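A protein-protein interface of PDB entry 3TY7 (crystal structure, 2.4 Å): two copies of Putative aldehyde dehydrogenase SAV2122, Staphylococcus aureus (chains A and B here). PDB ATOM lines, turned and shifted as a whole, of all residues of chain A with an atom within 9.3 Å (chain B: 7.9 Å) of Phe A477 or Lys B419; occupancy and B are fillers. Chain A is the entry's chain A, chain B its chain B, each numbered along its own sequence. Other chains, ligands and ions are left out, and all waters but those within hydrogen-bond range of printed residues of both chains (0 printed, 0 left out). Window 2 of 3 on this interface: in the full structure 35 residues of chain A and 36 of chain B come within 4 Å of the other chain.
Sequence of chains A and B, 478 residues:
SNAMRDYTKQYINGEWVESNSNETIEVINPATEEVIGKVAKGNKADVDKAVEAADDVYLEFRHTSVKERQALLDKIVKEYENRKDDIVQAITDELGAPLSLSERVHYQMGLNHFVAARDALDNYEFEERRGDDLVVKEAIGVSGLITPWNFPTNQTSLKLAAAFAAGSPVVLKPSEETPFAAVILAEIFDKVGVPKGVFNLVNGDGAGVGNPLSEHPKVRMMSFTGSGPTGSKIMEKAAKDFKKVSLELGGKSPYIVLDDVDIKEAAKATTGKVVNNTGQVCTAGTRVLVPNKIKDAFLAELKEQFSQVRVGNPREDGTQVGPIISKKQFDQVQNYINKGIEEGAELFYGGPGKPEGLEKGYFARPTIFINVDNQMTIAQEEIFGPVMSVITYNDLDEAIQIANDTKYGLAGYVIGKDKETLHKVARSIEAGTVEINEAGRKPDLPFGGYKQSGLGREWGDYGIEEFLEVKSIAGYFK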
ATOM      1  N   GLU A 127     -10.118   9.263 -18.637  1.00  0.00           N
ATOM      2  CA  GLU A 127     -11.060   9.053 -19.728  1.00  0.00           C
ATOM      3  C   GLU A 127     -11.040  10.219 -20.705  1.00  0.00           C
ATOM      4  O   GLU A 127     -11.070  11.383 -20.303  1.00  0.00           O
ATOM      5  CB  GLU A 127     -12.478   8.823 -19.200  1.00  0.00           C
ATOM      6  CG  GLU A 127     -12.603   7.624 -18.269  1.00  0.00           C
ATOM      7  CD  GLU A 127     -14.000   7.042 -18.238  1.00  0.00           C
ATOM      8  OE1 GLU A 127     -14.826   7.427 -19.091  1.00  0.00           O
ATOM      9  OE2 GLU A 127     -14.268   6.195 -17.359  1.00  0.00           O
ATOM     10  N   GLU A 128     -10.976   9.891 -21.990  1.00  0.00           N
ATOM     11  CA  GLU A 128     -10.945  10.893 -23.044  1.00  0.00           C
ATOM     12  C   GLU A 128     -11.802  10.427 -24.214  1.00  0.00           C
ATOM     13  O   GLU A 128     -11.682   9.288 -24.662  1.00  0.00           O
ATOM     14  CB  GLU A 128      -9.501  11.119 -23.498  1.00  0.00           C
ATOM     15  CG  GLU A 128      -9.333  12.121 -24.624  1.00  0.00           C
ATOM     16  CD  GLU A 128      -7.880  12.277 -25.035  1.00  0.00           C
ATOM     17  OE1 GLU A 128      -7.033  11.527 -24.504  1.00  0.00           O
ATOM     18  OE2 GLU A 128      -7.585  13.147 -25.881  1.00  0.00           O
ATOM     19  N   ARG A 129     -12.673  11.302 -24.702  1.00  0.00           N
ATOM     20  CA  ARG A 129     -13.504  10.963 -25.849  1.00  0.00           C
ATOM     21  C   ARG A 129     -12.841  11.396 -27.147  1.00  0.00           C
ATOM     22  O   ARG A 129     -12.405  12.540 -27.281  1.00  0.00           O
ATOM     23  CB  ARG A 129     -14.896  11.597 -25.747  1.00  0.00           C
ATOM     24  CG  ARG A 129     -15.680  11.526 -27.053  1.00  0.00           C
ATOM     25  CD  ARG A 129     -17.145  11.897 -26.890  1.00  0.00           C
ATOM     26  NE  ARG A 129     -17.878  11.707 -28.141  1.00  0.00           N
ATOM     27  CZ  ARG A 129     -19.198  11.809 -28.262  1.00  0.00           C
ATOM     28  NH1 ARG A 129     -19.776  11.620 -29.441  1.00  0.00           N
ATOM     29  NH2 ARG A 129     -19.940  12.099 -27.203  1.00  0.00           N
ATOM     30  N   ARG A 130     -12.752  10.471 -28.099  1.00  0.00           N
ATOM     31  CA  ARG A 130     -12.298  10.810 -29.440  1.00  0.00           C
ATOM     32  C   ARG A 130     -13.320  10.311 -30.448  1.00  0.00           C
ATOM     33  O   ARG A 130     -13.485   9.103 -30.630  1.00  0.00           O
ATOM     34  CB  ARG A 130     -10.932  10.181 -29.712  1.00  0.00           C
ATOM     35  CG  ARG A 130      -9.867  10.608 -28.722  1.00  0.00           C
ATOM     36  CD  ARG A 130      -8.547   9.919 -28.987  1.00  0.00           C
ATOM     37  NE  ARG A 130      -7.527  10.345 -28.035  1.00  0.00           N
ATOM     38  CZ  ARG A 130      -6.321   9.799 -27.938  1.00  0.00           C
ATOM     39  NH1 ARG A 130      -5.977   8.795 -28.734  1.00  0.00           N
ATOM     40  NH2 ARG A 130      -5.457  10.251 -27.040  1.00  0.00           N
ATOM     41  N   GLY A 131     -13.987  11.244 -31.118  1.00  0.00           N
ATOM     42  CA  GLY A 131     -15.067  10.897 -32.021  1.00  0.00           C
ATOM     43  C   GLY A 131     -16.128  10.081 -31.306  1.00  0.00           C
ATOM     44  O   GLY A 131     -16.662  10.490 -30.274  1.00  0.00           O
ATOM     45  N   ASP A 132     -16.420   8.910 -31.857  1.00  0.00           N
ATOM     46  CA  ASP A 132     -17.388   7.998 -31.268  1.00  0.00           C
ATOM     47  C   ASP A 132     -16.702   6.993 -30.352  1.00  0.00           C
ATOM     48  O   ASP A 132     -17.345   6.092 -29.815  1.00  0.00           O
ATOM     49  CB  ASP A 132     -18.148   7.276 -32.374  1.00  0.00           C
ATOM     50  CG  ASP A 132     -18.623   8.221 -33.453  1.00  0.00           C
ATOM     51  OD1 ASP A 132     -18.923   9.387 -33.120  1.00  0.00           O
ATOM     52  OD2 ASP A 132     -18.698   7.806 -34.628  1.00  0.00           O
ATOM     53  N   ASP A 133     -15.392   7.156 -30.178  1.00  0.00           N
ATOM     54  CA  ASP A 133     -14.593   6.220 -29.392  1.00  0.00           C
ATOM     55  C   ASP A 133     -14.226   6.798 -28.033  1.00  0.00           C
ATOM     56  O   ASP A 133     -14.040   8.008 -27.886  1.00  0.00           O
ATOM     57  CB  ASP A 133     -13.311   5.841 -30.141  1.00  0.00           C
ATOM     58  CG  ASP A 133     -13.583   5.349 -31.544  1.00  0.00           C
ATOM     59  OD1 ASP A 133     -14.604   4.659 -31.743  1.00  0.00           O
ATOM     60  OD2 ASP A 133     -12.782   5.661 -32.451  1.00  0.00           O
ATOM     61  N   LEU A 134     -14.132   5.918 -27.041  1.00  0.00           N
ATOM     62  CA  LEU A 134     -13.711   6.299 -25.702  1.00  0.00           C
ATOM     63  C   LEU A 134     -12.389   5.633 -25.333  1.00  0.00           C
ATOM     64  O   LEU A 134     -12.262   4.408 -25.375  1.00  0.00           O
ATOM     65  CB  LEU A 134     -14.783   5.916 -24.681  1.00  0.00           C
ATOM     66  CG  LEU A 134     -14.334   5.913 -23.216  1.00  0.00           C
ATOM     67  CD1 LEU A 134     -14.102   7.334 -22.720  1.00  0.00           C
ATOM     68  CD2 LEU A 134     -15.336   5.176 -22.336  1.00  0.00           C
ATOM     69  N   VAL A 135     -11.402   6.444 -24.973  1.00  0.00           N
ATOM     70  CA  VAL A 135     -10.128   5.924 -24.498  1.00  0.00           C
ATOM     71  C   VAL A 135     -10.076   6.007 -22.978  1.00  0.00           C
ATOM     72  O   VAL A 135     -10.278   7.077 -22.403  1.00  0.00           O
ATOM     73  CB  VAL A 135      -8.942   6.707 -25.088  1.00  0.00           C
ATOM     74  CG1 VAL A 135      -7.642   6.258 -24.443  1.00  0.00           C
ATOM     75  CG2 VAL A 135      -8.884   6.531 -26.598  1.00  0.00           C
ATOM     76  N   VAL A 136      -9.817   4.876 -22.331  1.00  0.00           N
ATOM     77  CA  VAL A 136      -9.725   4.840 -20.876  1.00  0.00           C
ATOM     78  C   VAL A 136      -8.361   4.354 -20.400  1.00  0.00           C
ATOM     79  O   VAL A 136      -7.659   3.627 -21.106  1.00  0.00           O
ATOM     80  CB  VAL A 136     -10.815   3.939 -20.249  1.00  0.00           C
ATOM     81  CG1 VAL A 136     -12.192   4.389 -20.682  1.00  0.00           C
ATOM     82  CG2 VAL A 136     -10.595   2.491 -20.633  1.00  0.00           C
ATOM     83  N   ILE A 473     -12.106   1.942 -26.546  1.00  0.00           N
ATOM     84  CA  ILE A 473     -13.367   1.295 -26.869  1.00  0.00           C
ATOM     85  C   ILE A 473     -13.953   1.951 -28.109  1.00  0.00           C
ATOM     86  O   ILE A 473     -14.388   3.102 -28.064  1.00  0.00           O
ATOM     87  CB  ILE A 473     -14.372   1.414 -25.713  1.00  0.00           C
ATOM     88  CG1 ILE A 473     -13.757   0.892 -24.410  1.00  0.00           C
ATOM     89  CG2 ILE A 473     -15.657   0.667 -26.047  1.00  0.00           C
ATOM     90  CD1 ILE A 473     -14.654   1.064 -23.202  1.00  0.00           C
ATOM     91  N   ALA A 474     -13.965   1.214 -29.214  1.00  0.00           N
ATOM     92  CA  ALA A 474     -14.421   1.761 -30.486  1.00  0.00           C
ATOM     93  C   ALA A 474     -15.942   1.733 -30.629  1.00  0.00           C
ATOM     94  O   ALA A 474     -16.581   0.702 -30.424  1.00  0.00           O
ATOM     95  CB  ALA A 474     -13.762   1.029 -31.645  1.00  0.00           C
ATOM     96  N   GLY A 475     -16.513   2.880 -30.981  1.00  0.00           N
ATOM     97  CA  GLY A 475     -17.941   2.986 -31.210  1.00  0.00           C
ATOM     98  C   GLY A 475     -18.737   3.094 -29.928  1.00  0.00           C
ATOM     99  O   GLY A 475     -19.937   2.817 -29.908  1.00  0.00           O
ATOM    100  N   TYR A 476     -18.072   3.517 -28.857  1.00  0.00           N
ATOM    101  CA  TYR A 476     -18.724   3.654 -27.561  1.00  0.00           C
ATOM    102  C   TYR A 476     -19.929   4.592 -27.641  1.00  0.00           C
ATOM    103  O   TYR A 476     -21.024   4.250 -27.203  1.00  0.00           O
ATOM    104  CB  TYR A 476     -17.728   4.165 -26.516  1.00  0.00           C
ATOM    105  CG  TYR A 476     -18.270   4.177 -25.104  1.00  0.00           C
ATOM    106  CD1 TYR A 476     -18.184   3.052 -24.296  1.00  0.00           C
ATOM    107  CD2 TYR A 476     -18.868   5.317 -24.578  1.00  0.00           C
ATOM    108  CE1 TYR A 476     -18.677   3.059 -23.004  1.00  0.00           C
ATOM    109  CE2 TYR A 476     -19.366   5.334 -23.288  1.00  0.00           C
ATOM    110  CZ  TYR A 476     -19.269   4.204 -22.504  1.00  0.00           C
ATOM    111  OH  TYR A 476     -19.762   4.215 -21.219  1.00  0.00           O
ATOM    112  N   PHE A 477     -19.723   5.771 -28.216  1.00  0.00           N
ATOM    113  CA  PHE A 477     -20.743   6.815 -28.204  1.00  0.00           C
ATOM    114  C   PHE A 477     -21.861   6.654 -29.239  1.00  0.00           C
ATOM    115  O   PHE A 477     -23.025   6.911 -28.934  1.00  0.00           O
ATOM    116  CB  PHE A 477     -20.085   8.194 -28.281  1.00  0.00           C
ATOM    117  CG  PHE A 477     -19.196   8.491 -27.108  1.00  0.00           C
ATOM    118  CD1 PHE A 477     -19.717   9.048 -25.951  1.00  0.00           C
ATOM    119  CD2 PHE A 477     -17.845   8.193 -27.152  1.00  0.00           C
ATOM    120  CE1 PHE A 477     -18.904   9.315 -24.865  1.00  0.00           C
ATOM    121  CE2 PHE A 477     -17.026   8.454 -26.068  1.00  0.00           C
ATOM    122  CZ  PHE A 477     -17.556   9.018 -24.924  1.00  0.00           C
ATOM    123  N   LYS A 478     -21.518   6.240 -30.454  1.00  0.00           N
ATOM    124  CA  LYS A 478     -22.539   6.025 -31.478  1.00  0.00           C
ATOM    125  C   LYS A 478     -23.436   4.839 -31.138  1.00  0.00           C
ATOM    126  O   LYS A 478     -24.662   4.948 -31.175  1.00  0.00           O
ATOM    127  CB  LYS A 478     -21.912   5.828 -32.859  1.00  0.00           C
ATOM    128  CG  LYS A 478     -21.691   7.118 -33.636  1.00  0.00           C
ATOM    129  CD  LYS A 478     -22.989   7.865 -33.917  1.00  0.00           C
ATOM    130  CE  LYS A 478     -22.723   9.122 -34.734  1.00  0.00           C
ATOM    131  NZ  LYS A 478     -23.979   9.847 -35.066  1.00  0.00           N
ATOM    132  N   LEU B 258     -24.871 -10.386 -27.526  1.00  0.00           N
ATOM    133  CA  LEU B 258     -26.024 -10.137 -26.666  1.00  0.00           C
ATOM    134  C   LEU B 258     -27.269 -10.836 -27.206  1.00  0.00           C
ATOM    135  O   LEU B 258     -27.362 -11.107 -28.402  1.00  0.00           O
ATOM    136  CB  LEU B 258     -26.276  -8.638 -26.522  1.00  0.00           C
ATOM    137  CG  LEU B 258     -25.148  -7.829 -25.881  1.00  0.00           C
ATOM    138  CD1 LEU B 258     -25.582  -6.383 -25.692  1.00  0.00           C
ATOM    139  CD2 LEU B 258     -24.717  -8.451 -24.561  1.00  0.00           C
ATOM    140  N   ASP B 260     -30.208  -9.659 -27.527  1.00  0.00           N
ATOM    141  CA  ASP B 260     -31.074  -8.749 -28.277  1.00  0.00           C
ATOM    142  C   ASP B 260     -30.532  -8.444 -29.671  1.00  0.00           C
ATOM    143  O   ASP B 260     -31.107  -7.646 -30.409  1.00  0.00           O
ATOM    144  CB  ASP B 260     -31.323  -7.450 -27.501  1.00  0.00           C
ATOM    145  CG  ASP B 260     -30.040  -6.785 -27.036  1.00  0.00           C
ATOM    146  OD1 ASP B 260     -28.959  -7.104 -27.578  1.00  0.00           O
ATOM    147  OD2 ASP B 260     -30.117  -5.934 -26.122  1.00  0.00           O
ATOM    148  N   GLY B 416     -24.549  -6.065 -29.987  1.00  0.00           N
ATOM    149  CA  GLY B 416     -25.880  -6.078 -29.415  1.00  0.00           C
ATOM    150  C   GLY B 416     -26.628  -4.783 -29.649  1.00  0.00           C
ATOM    151  O   GLY B 416     -26.239  -3.969 -30.489  1.00  0.00           O
ATOM    152  N   LYS B 417     -27.703  -4.595 -28.895  1.00  0.00           N
ATOM    153  CA  LYS B 417     -28.578  -3.442 -29.072  1.00  0.00           C
ATOM    154  C   LYS B 417     -28.594  -2.490 -27.874  1.00  0.00           C
ATOM    155  O   LYS B 417     -28.228  -1.322 -28.011  1.00  0.00           O
ATOM    156  CB  LYS B 417     -29.987  -3.882 -29.475  1.00  0.00           C
ATOM    157  CG  LYS B 417     -30.082  -4.262 -30.948  1.00  0.00           C
ATOM    158  CD  LYS B 417     -31.498  -4.623 -31.360  1.00  0.00           C
ATOM    159  CE  LYS B 417     -31.646  -4.596 -32.873  1.00  0.00           C
ATOM    160  NZ  LYS B 417     -30.547  -5.336 -33.557  1.00  0.00           N
ATOM    161  N   ASP B 418     -29.038  -2.983 -26.719  1.00  0.00           N
ATOM    162  CA  ASP B 418     -29.125  -2.157 -25.514  1.00  0.00           C
ATOM    163  C   ASP B 418     -27.785  -1.505 -25.186  1.00  0.00           C
ATOM    164  O   ASP B 418     -26.768  -2.181 -25.049  1.00  0.00           O
ATOM    165  CB  ASP B 418     -29.595  -2.990 -24.320  1.00  0.00           C
ATOM    166  CG  ASP B 418     -29.785  -2.153 -23.066  1.00  0.00           C
ATOM    167  OD1 ASP B 418     -30.483  -1.120 -23.140  1.00  0.00           O
ATOM    168  OD2 ASP B 418     -29.228  -2.523 -22.011  1.00  0.00           O
ATOM    169  N   LYS B 419     -27.812  -0.185 -25.036  1.00  0.00           N
ATOM    170  CA  LYS B 419     -26.600   0.623 -24.967  1.00  0.00           C
ATOM    171  C   LYS B 419     -25.885   0.514 -23.623  1.00  0.00           C
ATOM    172  O   LYS B 419     -24.655   0.513 -23.568  1.00  0.00           O
ATOM    173  CB  LYS B 419     -26.941   2.082 -25.280  1.00  0.00           C
ATOM    174  CG  LYS B 419     -25.752   2.989 -25.555  1.00  0.00           C
ATOM    175  CD  LYS B 419     -26.238   4.345 -26.058  1.00  0.00           C
ATOM    176  CE  LYS B 419     -25.170   5.425 -25.942  1.00  0.00           C
ATOM    177  NZ  LYS B 419     -24.059   5.252 -26.919  1.00  0.00           N
ATOM    178  N   GLU B 420     -26.655   0.426 -22.544  1.00  0.00           N
ATOM    179  CA  GLU B 420     -26.081   0.301 -21.208  1.00  0.00           C
ATOM    180  C   GLU B 420     -25.390  -1.050 -21.074  1.00  0.00           C
ATOM    181  O   GLU B 420     -24.329  -1.165 -20.459  1.00  0.00           O
ATOM    182  CB  GLU B 420     -27.169   0.431 -20.139  1.00  0.00           C
ATOM    183  CG  GLU B 420     -28.416   1.180 -20.589  1.00  0.00           C
ATOM    184  CD  GLU B 420     -28.168   2.658 -20.836  1.00  0.00           C
ATOM    185  OE1 GLU B 420     -27.159   3.190 -20.326  1.00  0.00           O
ATOM    186  OE2 GLU B 420     -28.986   3.286 -21.542  1.00  0.00           O
ATOM    187  N   THR B 421     -26.011  -2.070 -21.656  1.00  0.00           N
ATOM    188  CA  THR B 421     -25.474  -3.422 -21.630  1.00  0.00           C
ATOM    189  C   THR B 421     -24.174  -3.497 -22.423  1.00  0.00           C
ATOM    190  O   THR B 421     -23.207  -4.121 -21.989  1.00  0.00           O
ATOM    191  CB  THR B 421     -26.483  -4.427 -22.211  1.00  0.00           C
ATOM    192  OG1 THR B 421     -27.708  -4.358 -21.471  1.00  0.00           O
ATOM    193  CG2 THR B 421     -25.936  -5.836 -22.137  1.00  0.00           C
ATOM    194  N   LEU B 422     -24.159  -2.850 -23.583  1.00  0.00           N
ATOM    195  CA  LEU B 422     -22.965  -2.788 -24.416  1.00  0.00           C
ATOM    196  C   LEU B 422     -21.816  -2.095 -23.689  1.00  0.00           C
ATOM    197  O   LEU B 422     -20.685  -2.582 -23.696  1.00  0.00           O
ATOM    198  CB  LEU B 422     -23.268  -2.070 -25.733  1.00  0.00           C
ATOM    199  CG  LEU B 422     -24.141  -2.837 -26.729  1.00  0.00           C
ATOM    200  CD1 LEU B 422     -24.627  -1.925 -27.851  1.00  0.00           C
ATOM    201  CD2 LEU B 422     -23.383  -4.030 -27.292  1.00  0.00           C
ATOM    202  N   HIS B 423     -22.117  -0.963 -23.063  1.00  0.00           N
ATOM    203  CA  HIS B 423     -21.124  -0.201 -22.313  1.00  0.00           C
ATOM    204  C   HIS B 423     -20.502  -1.011 -21.185  1.00  0.00           C
ATOM    205  O   HIS B 423     -19.283  -1.012 -21.012  1.00  0.00           O
ATOM    206  CB  HIS B 423     -21.753   1.068 -21.735  1.00  0.00           C
ATOM    207  CG  HIS B 423     -22.084   2.099 -22.766  1.00  0.00           C
ATOM    208  ND1 HIS B 423     -21.541   2.085 -24.031  1.00  0.00           N
ATOM    209  CD2 HIS B 423     -22.905   3.176 -22.718  1.00  0.00           C
ATOM    210  CE1 HIS B 423     -22.011   3.110 -24.720  1.00  0.00           C
ATOM    211  NE2 HIS B 423     -22.840   3.787 -23.946  1.00  0.00           N
ATOM    212  N   LYS B 424     -21.349  -1.688 -20.418  1.00  0.00           N
ATOM    213  CA  LYS B 424     -20.895  -2.483 -19.283  1.00  0.00           C
ATOM    214  C   LYS B 424     -19.983  -3.620 -19.733  1.00  0.00           C
ATOM    215  O   LYS B 424     -18.905  -3.823 -19.170  1.00  0.00           O
ATOM    216  CB  LYS B 424     -22.092  -3.043 -18.510  1.00  0.00           C
ATOM    217  CG  LYS B 424     -21.712  -3.933 -17.338  1.00  0.00           C
ATOM    218  CD  LYS B 424     -22.906  -4.733 -16.844  1.00  0.00           C
ATOM    219  CE  LYS B 424     -22.475  -5.837 -15.894  1.00  0.00           C
ATOM    220  NZ  LYS B 424     -23.574  -6.810 -15.657  1.00  0.00           N
ATOM    221  N   VAL B 425     -20.423  -4.356 -20.748  1.00  0.00           N
ATOM    222  CA  VAL B 425     -19.624  -5.435 -21.310  1.00  0.00           C
ATOM    223  C   VAL B 425     -18.290  -4.909 -21.829  1.00  0.00           C
ATOM    224  O   VAL B 425     -17.233  -5.463 -21.519  1.00  0.00           O
ATOM    225  CB  VAL B 425     -20.366  -6.153 -22.455  1.00  0.00           C
ATOM    226  CG1 VAL B 425     -19.434  -7.119 -23.157  1.00  0.00           C
ATOM    227  CG2 VAL B 425     -21.585  -6.883 -21.917  1.00  0.00           C
ATOM    228  N   ALA B 426     -18.350  -3.833 -22.608  1.00  0.00           N
ATOM    229  CA  ALA B 426     -17.155  -3.208 -23.168  1.00  0.00           C
ATOM    230  C   ALA B 426     -16.155  -2.825 -22.080  1.00  0.00           C
ATOM    231  O   ALA B 426     -14.954  -3.063 -22.215  1.00  0.00           O
ATOM    232  CB  ALA B 426     -17.531  -1.985 -23.997  1.00  0.00           C
ATOM    233  N   ARG B 427     -16.663  -2.238 -21.000  1.00  0.00           N
ATOM    234  CA  ARG B 427     -15.818  -1.815 -19.889  1.00  0.00           C
ATOM    235  C   ARG B 427     -15.317  -2.998 -19.060  1.00  0.00           C
ATOM    236  O   ARG B 427     -14.254  -2.923 -18.442  1.00  0.00           O
ATOM    237  CB  ARG B 427     -16.563  -0.824 -18.990  1.00  0.00           C
ATOM    238  CG  ARG B 427     -16.698   0.584 -19.563  1.00  0.00           C
ATOM    239  CD  ARG B 427     -17.410   1.498 -18.576  1.00  0.00           C
ATOM    240  NE  ARG B 427     -17.432   2.897 -19.002  1.00  0.00           N
ATOM    241  CZ  ARG B 427     -16.461   3.768 -18.747  1.00  0.00           C
ATOM    242  NH1 ARG B 427     -16.563   5.023 -19.167  1.00  0.00           N
ATOM    243  NH2 ARG B 427     -15.383   3.383 -18.075  1.00  0.00           N
ATOM    244  N   ILE B 436     -17.312  -2.236 -30.185  1.00  0.00           N
ATOM    245  CA  ILE B 436     -18.759  -2.358 -30.044  1.00  0.00           C
ATOM    246  C   ILE B 436     -19.440  -2.288 -31.405  1.00  0.00           C
ATOM    247  O   ILE B 436     -19.279  -1.310 -32.133  1.00  0.00           O
ATOM    248  CB  ILE B 436     -19.343  -1.238 -29.149  1.00  0.00           C
ATOM    249  CG1 ILE B 436     -18.747  -1.305 -27.742  1.00  0.00           C
ATOM    250  CG2 ILE B 436     -20.863  -1.334 -29.090  1.00  0.00           C
ATOM    251  CD1 ILE B 436     -19.237  -0.207 -26.819  1.00  0.00           C
ATOM    252  N   ASN B 437     -20.196  -3.330 -31.738  1.00  0.00           N
ATOM    253  CA  ASN B 437     -20.960  -3.382 -32.985  1.00  0.00           C
ATOM    254  C   ASN B 437     -20.156  -3.082 -34.250  1.00  0.00           C
ATOM    255  O   ASN B 437     -20.585  -2.288 -35.088  1.00  0.00           O
ATOM    256  CB  ASN B 437     -22.179  -2.459 -32.910  1.00  0.00           C
ATOM    257  CG  ASN B 437     -23.249  -2.984 -31.976  1.00  0.00           C
ATOM    258  OD1 ASN B 437     -23.380  -4.191 -31.782  1.00  0.00           O
ATOM    259  ND2 ASN B 437     -24.024  -2.077 -31.392  1.00  0.00           N
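Of the printed residues of chain B, Ile A473 touches Ala B426 and Ile B436. Of the printed residues of chain B, Tyr A476 touches Lys B419 (3.2 Å), His B423 (2.9 Å), Arg B427 (3.5 Å) and Ile B436 (3.96 Å). No residue of chain A comes within 4 Å of Asp B418. Lys B419 touches two residues of chain A. No residue of chain A comes within 4 Å of Glu B420. Leu B422 touches none of the printed residues of chain A. Printed residues of chain A within 4 Å of Ala B426: Ile A473. The nearest residue of chain B that does not touch Phe A477 is His B423 (5.0 Å). The nearest residue of chain A that does not touch Lys B419 is Lys A478 (4.3 Å). The nearest printed residue of chain A that does not touch Ile B436 is Gly A475 (4.2 Å).
Among the printed residues, pairs that only touch across the chains: Leu A134 with Arg B427 (3.4 Å), Ile A473 with Ala B426 (3.8 Å), Ile A473 with Ile B436 (3.8 Å), Tyr A476 with His B423 (2.9 Å) and Tyr A476 with Ile B436 (3.96 Å).
Of the 16 printed residues of chain B, 5 touch a printed residue of chain A. Along chain B the printed residues that touch a printed residue of chain A span positions 419 to 436. Printed residues of chain A that touch a printed residue of chain B: Glu A127, Leu A134, Ile A473, Ala A474, Tyr A476 and Phe A477. Hydrophobic or aromatic side chains of chain A that line the printed part of chain B: Leu A134, Ile A473 and Tyr A476. Among the printed residues, Asp or Glu carboxylates within 4 Å of a Lys or Arg side-chain nitrogen of the other chain: Glu A127 with Arg B427.
No position is printed for both chains. Of the 10 pairs that touch across the chains among the printed residues, none has its exchanged pair printed and touching as well.
The guanidinium group of Arg B427 lies within hydrogen-bond range of the side-chain hydroxyl of Tyr A476 (3.5 Å). O of Ala A474 sits at hydrogen-bond distance from N of Ile B436 (3.0 Å). The side-chain amino group of Lys B419 sits at hydrogen-bond distance from the backbone carbonyl oxygen of Tyr A476, at 3.2 Å. NH1 of Arg B427 is in salt-bridge range of OE1 of Glu A127. The backbone carbonyl oxygen (O) of Phe A477 lies within hydrogen-bond range of the side-chain amino group (NZ) of Lys B419 (2.8 Å).
The backbone carbonyl oxygen (O) of Leu A134 is in hydrogen-bond range of the backbone NH (N) of Ile A473. The backbone carbonyl oxygen (O) of Asp A132 is in hydrogen-bond range of the backbone NH (N) of Phe A477 (2.9 Å). The backbone NH (N) of Tyr A476 lies within hydrogen-bond range of the backbone carbonyl oxygen (O) of Asp A132, at 2.8 Å.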
